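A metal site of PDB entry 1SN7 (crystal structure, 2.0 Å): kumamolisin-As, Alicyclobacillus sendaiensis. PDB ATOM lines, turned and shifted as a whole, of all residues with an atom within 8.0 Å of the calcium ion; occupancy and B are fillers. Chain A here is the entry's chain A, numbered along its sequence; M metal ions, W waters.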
ATOM      1  N   VAL A 207      -8.667  22.804  -5.034  1.00  0.00           N
ATOM      2  CA  VAL A 207      -7.206  22.756  -4.870  1.00  0.00           C
ATOM      3  C   VAL A 207      -6.799  21.484  -4.174  1.00  0.00           C
ATOM      4  O   VAL A 207      -7.457  21.161  -3.153  1.00  0.00           O
ATOM      5  CB  VAL A 207      -6.758  23.982  -4.058  1.00  0.00           C
ATOM      6  CG1 VAL A 207      -5.251  24.033  -3.830  1.00  0.00           C
ATOM      7  CG2 VAL A 207      -7.263  25.240  -4.771  1.00  0.00           C
ATOM      8  N   HIS A 315     -12.036  24.517 -17.161  1.00  0.00           N
ATOM      9  CA  HIS A 315     -12.858  24.363 -15.971  1.00  0.00           C
ATOM     10  C   HIS A 315     -12.173  25.107 -14.812  1.00  0.00           C
ATOM     11  O   HIS A 315     -11.125  24.688 -14.314  1.00  0.00           O
ATOM     12  CB  HIS A 315     -13.028  22.913 -15.574  1.00  0.00           C
ATOM     13  CG  HIS A 315     -13.959  22.756 -14.425  1.00  0.00           C
ATOM     14  ND1 HIS A 315     -13.549  22.477 -13.150  1.00  0.00           N
ATOM     15  CD2 HIS A 315     -15.314  22.838 -14.379  1.00  0.00           C
ATOM     16  CE1 HIS A 315     -14.609  22.385 -12.352  1.00  0.00           C
ATOM     17  NE2 HIS A 315     -15.681  22.612 -13.080  1.00  0.00           N
ATOM     18  N   ASP A 316     -12.716  26.204 -14.345  1.00  0.00           N
ATOM     19  CA  ASP A 316     -12.115  27.033 -13.305  1.00  0.00           C
ATOM     20  C   ASP A 316     -12.183  26.417 -11.924  1.00  0.00           C
ATOM     21  O   ASP A 316     -13.267  25.996 -11.521  1.00  0.00           O
ATOM     22  CB  ASP A 316     -12.881  28.357 -13.326  1.00  0.00           C
ATOM     23  CG  ASP A 316     -12.204  29.432 -12.501  1.00  0.00           C
ATOM     24  OD1 ASP A 316     -11.159  29.121 -11.881  1.00  0.00           O
ATOM     25  OD2 ASP A 316     -12.749  30.560 -12.522  1.00  0.00           O
ATOM     26  N   ILE A 317     -11.095  26.336 -11.175  1.00  0.00           N
ATOM     27  CA  ILE A 317     -11.164  25.871  -9.804  1.00  0.00           C
ATOM     28  C   ILE A 317     -11.221  27.156  -8.985  1.00  0.00           C
ATOM     29  O   ILE A 317     -10.418  28.075  -9.275  1.00  0.00           O
ATOM     30  CB  ILE A 317      -9.979  24.991  -9.389  1.00  0.00           C
ATOM     31  CG1 ILE A 317     -10.031  23.587  -9.973  1.00  0.00           C
ATOM     32  CG2 ILE A 317      -9.860  24.954  -7.860  1.00  0.00           C
ATOM     33  CD1 ILE A 317      -9.576  23.444 -11.404  1.00  0.00           C
ATOM     34  N   THR A 318     -12.147  27.209  -8.008  1.00  0.00           N
ATOM     35  CA  THR A 318     -12.242  28.485  -7.297  1.00  0.00           C
ATOM     36  C   THR A 318     -12.224  28.314  -5.786  1.00  0.00           C
ATOM     37  O   THR A 318     -12.281  29.266  -5.063  1.00  0.00           O
ATOM     38  CB  THR A 318     -13.561  29.221  -7.572  1.00  0.00           C
ATOM     39  OG1 THR A 318     -14.639  28.354  -7.161  1.00  0.00           O
ATOM     40  CG2 THR A 318     -13.799  29.501  -9.048  1.00  0.00           C
ATOM     41  N   GLU A 319     -12.153  27.076  -5.325  1.00  0.00           N
ATOM     42  CA  GLU A 319     -12.221  26.814  -3.906  1.00  0.00           C
ATOM     43  C   GLU A 319     -11.009  26.083  -3.376  1.00  0.00           C
ATOM     44  O   GLU A 319     -10.596  25.085  -3.985  1.00  0.00           O
ATOM     45  CB  GLU A 319     -13.491  25.951  -3.628  1.00  0.00           C
ATOM     46  CG  GLU A 319     -13.185  24.899  -2.593  1.00  0.00           C
ATOM     47  CD  GLU A 319     -14.424  24.312  -1.941  1.00  0.00           C
ATOM     48  OE1 GLU A 319     -15.520  24.477  -2.534  1.00  0.00           O
ATOM     49  OE2 GLU A 319     -14.280  23.713  -0.856  1.00  0.00           O
ATOM     50  N   GLN A 332      -4.625  31.198  -2.243  1.00  0.00           N
ATOM     51  CA  GLN A 332      -6.024  30.831  -2.381  1.00  0.00           C
ATOM     52  C   GLN A 332      -6.500  30.698  -3.824  1.00  0.00           C
ATOM     53  O   GLN A 332      -6.046  31.508  -4.648  1.00  0.00           O
ATOM     54  CB  GLN A 332      -6.919  31.904  -1.704  1.00  0.00           C
ATOM     55  CG  GLN A 332      -7.166  31.395  -0.284  1.00  0.00           C
ATOM     56  CD  GLN A 332      -8.590  31.716   0.134  1.00  0.00           C
ATOM     57  OE1 GLN A 332      -9.389  30.803   0.326  1.00  0.00           O
ATOM     58  NE2 GLN A 332      -8.880  33.018   0.248  1.00  0.00           N
ATOM     59  N   ALA A 333      -7.363  29.720  -4.093  1.00  0.00           N
ATOM     60  CA  ALA A 333      -7.851  29.623  -5.485  1.00  0.00           C
ATOM     61  C   ALA A 333      -8.925  30.704  -5.625  1.00  0.00           C
ATOM     62  O   ALA A 333      -9.402  31.199  -4.587  1.00  0.00           O
ATOM     63  CB  ALA A 333      -8.365  28.255  -5.876  1.00  0.00           C
ATOM     64  N   GLY A 334      -9.311  31.104  -6.826  1.00  0.00           N
ATOM     65  CA  GLY A 334     -10.334  32.150  -6.919  1.00  0.00           C
ATOM     66  C   GLY A 334     -10.919  32.122  -8.316  1.00  0.00           C
ATOM     67  O   GLY A 334     -10.429  31.279  -9.059  1.00  0.00           O
ATOM     68  N   PRO A 335     -11.897  32.946  -8.691  1.00  0.00           N
ATOM     69  CA  PRO A 335     -12.366  32.946 -10.097  1.00  0.00           C
ATOM     70  C   PRO A 335     -11.229  33.344 -11.040  1.00  0.00           C
ATOM     71  O   PRO A 335     -10.484  34.290 -10.802  1.00  0.00           O
ATOM     72  CB  PRO A 335     -13.514  33.963 -10.094  1.00  0.00           C
ATOM     73  CG  PRO A 335     -13.856  34.236  -8.683  1.00  0.00           C
ATOM     74  CD  PRO A 335     -12.643  33.897  -7.847  1.00  0.00           C
ATOM     75  N   GLY A 336     -11.048  32.638 -12.166  1.00  0.00           N
ATOM     76  CA  GLY A 336      -9.973  33.021 -13.069  1.00  0.00           C
ATOM     77  C   GLY A 336      -8.637  32.390 -12.658  1.00  0.00           C
ATOM     78  O   GLY A 336      -8.616  31.455 -11.852  1.00  0.00           O
ATOM     79  N   TRP A 337      -7.541  32.890 -13.210  1.00  0.00           N
ATOM     80  CA  TRP A 337      -6.195  32.476 -12.889  1.00  0.00           C
ATOM     81  C   TRP A 337      -5.974  32.628 -11.386  1.00  0.00           C
ATOM     82  O   TRP A 337      -6.325  33.695 -10.864  1.00  0.00           O
ATOM     83  CB  TRP A 337      -5.085  33.296 -13.593  1.00  0.00           C
ATOM     84  CG  TRP A 337      -3.735  32.630 -13.389  1.00  0.00           C
ATOM     85  CD1 TRP A 337      -3.151  31.712 -14.227  1.00  0.00           C
ATOM     86  CD2 TRP A 337      -2.817  32.820 -12.308  1.00  0.00           C
ATOM     87  NE1 TRP A 337      -1.924  31.324 -13.727  1.00  0.00           N
ATOM     88  CE2 TRP A 337      -1.700  31.983 -12.551  1.00  0.00           C
ATOM     89  CE3 TRP A 337      -2.850  33.630 -11.148  1.00  0.00           C
ATOM     90  CZ2 TRP A 337      -0.632  31.930 -11.676  1.00  0.00           C
ATOM     91  CZ3 TRP A 337      -1.790  33.589 -10.256  1.00  0.00           C
ATOM     92  CH2 TRP A 337      -0.716  32.735 -10.568  1.00  0.00           C
ATOM     93  N   ASP A 338      -5.368  31.653 -10.724  1.00  0.00           N
ATOM     94  CA  ASP A 338      -4.958  31.789  -9.323  1.00  0.00           C
ATOM     95  C   ASP A 338      -3.667  30.990  -9.075  1.00  0.00           C
ATOM     96  O   ASP A 338      -3.353  30.137  -9.896  1.00  0.00           O
ATOM     97  CB  ASP A 338      -6.042  31.340  -8.356  1.00  0.00           C
ATOM     98  CG  ASP A 338      -6.504  29.907  -8.533  1.00  0.00           C
ATOM     99  OD1 ASP A 338      -5.733  28.952  -8.258  1.00  0.00           O
ATOM    100  OD2 ASP A 338      -7.665  29.757  -8.955  1.00  0.00           O
ATOM    101  N   PRO A 339      -2.937  31.279  -8.002  1.00  0.00           N
ATOM    102  CA  PRO A 339      -1.643  30.627  -7.736  1.00  0.00           C
ATOM    103  C   PRO A 339      -1.722  29.192  -7.195  1.00  0.00           C
ATOM    104  O   PRO A 339      -0.699  28.696  -6.690  1.00  0.00           O
ATOM    105  CB  PRO A 339      -0.997  31.552  -6.689  1.00  0.00           C
ATOM    106  CG  PRO A 339      -1.851  32.779  -6.582  1.00  0.00           C
ATOM    107  CD  PRO A 339      -3.223  32.271  -6.938  1.00  0.00           C
ATOM    108  N   CYS A 340      -2.865  28.514  -7.301  1.00  0.00           N
ATOM    109  CA  CYS A 340      -2.954  27.123  -6.912  1.00  0.00           C
ATOM    110  C   CYS A 340      -3.202  26.224  -8.140  1.00  0.00           C
ATOM    111  O   CYS A 340      -2.613  25.132  -8.183  1.00  0.00           O
ATOM    112  CB  CYS A 340      -4.074  26.818  -5.902  1.00  0.00           C
ATOM    113  SG  CYS A 340      -4.083  27.943  -4.474  1.00  0.00           S
ATOM    114  N   THR A 341      -4.042  26.676  -9.089  1.00  0.00           N
ATOM    115  CA  THR A 341      -4.485  25.855 -10.199  1.00  0.00           C
ATOM    116  C   THR A 341      -4.374  26.551 -11.562  1.00  0.00           C
ATOM    117  O   THR A 341      -4.800  25.986 -12.563  1.00  0.00           O
ATOM    118  CB  THR A 341      -5.962  25.413 -10.050  1.00  0.00           C
ATOM    119  OG1 THR A 341      -6.757  26.608  -9.906  1.00  0.00           O
ATOM    120  CG2 THR A 341      -6.178  24.541  -8.816  1.00  0.00           C
ATOM    121  N   GLY A 342      -3.812  27.739 -11.586  1.00  0.00           N
ATOM    122  CA  GLY A 342      -3.606  28.517 -12.817  1.00  0.00           C
ATOM    123  C   GLY A 342      -4.897  28.812 -13.534  1.00  0.00           C
ATOM    124  O   GLY A 342      -5.836  29.328 -12.949  1.00  0.00           O
ATOM    125  N   LEU A 343      -4.977  28.480 -14.830  1.00  0.00           N
ATOM    126  CA  LEU A 343      -6.221  28.729 -15.537  1.00  0.00           C
ATOM    127  C   LEU A 343      -7.253  27.666 -15.210  1.00  0.00           C
ATOM    128  O   LEU A 343      -8.428  27.761 -15.562  1.00  0.00           O
ATOM    129  CB  LEU A 343      -5.949  28.790 -17.057  1.00  0.00           C
ATOM    130  CG  LEU A 343      -5.073  29.901 -17.622  1.00  0.00           C
ATOM    131  CD1 LEU A 343      -4.628  29.490 -19.040  1.00  0.00           C
ATOM    132  CD2 LEU A 343      -5.793  31.251 -17.596  1.00  0.00           C
ATOM    133  N   GLY A 344      -6.889  26.596 -14.511  1.00  0.00           N
ATOM    134  CA  GLY A 344      -7.856  25.552 -14.200  1.00  0.00           C
ATOM    135  C   GLY A 344      -7.505  24.281 -14.969  1.00  0.00           C
ATOM    136  O   GLY A 344      -6.389  24.159 -15.502  1.00  0.00           O
ATOM    137  N   SER A 345      -8.445  23.343 -15.049  1.00  0.00           N
ATOM    138  CA  SER A 345      -8.263  22.110 -15.825  1.00  0.00           C
ATOM    139  C   SER A 345      -8.794  22.366 -17.242  1.00  0.00           C
ATOM    140  O   SER A 345      -9.845  22.977 -17.406  1.00  0.00           O
ATOM    141  CB  SER A 345      -8.954  20.890 -15.229  1.00  0.00           C
ATOM    142  OG  SER A 345     -10.345  21.079 -15.087  1.00  0.00           O
HETATM  143 CA    CA M   1      -9.412  29.775 -10.505  1.00  0.00          CA
HETATM  144  O   HOH W   1      -8.458  27.967 -11.607  1.00  0.00           O
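The calcium ion is bound by O of Gly 336 (2.3 Å), OD1 of Asp 316 (2.3 Å), O of Gly 334 (2.3 Å), water W1 (2.3 Å), O of Ile 317 (2.3 Å) and OD2 of Asp 338 (2.3 Å). The calcium ion has six donor atoms within binding distance.
N of Thr 341 is in hydrogen-bond range of OD1 of Asp 338 (3.0 Å). The side-chain carboxylate of Asp 338 is in hydrogen-bond range of the backbone NH of Cys 340.
Water W1 lies within hydrogen-bond range of the side-chain hydroxyl of Thr 341 (2.8 Å), the backbone NH of Ile 317 (3.1 Å) and the backbone carbonyl oxygen of Gly 342 (3.2 Å).
Of the 20 residues printed, 5 come within 4 Å of the calcium ion. The nearest printed residue that does not touch the calcium ion is Pro 335 (4.04 Å).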
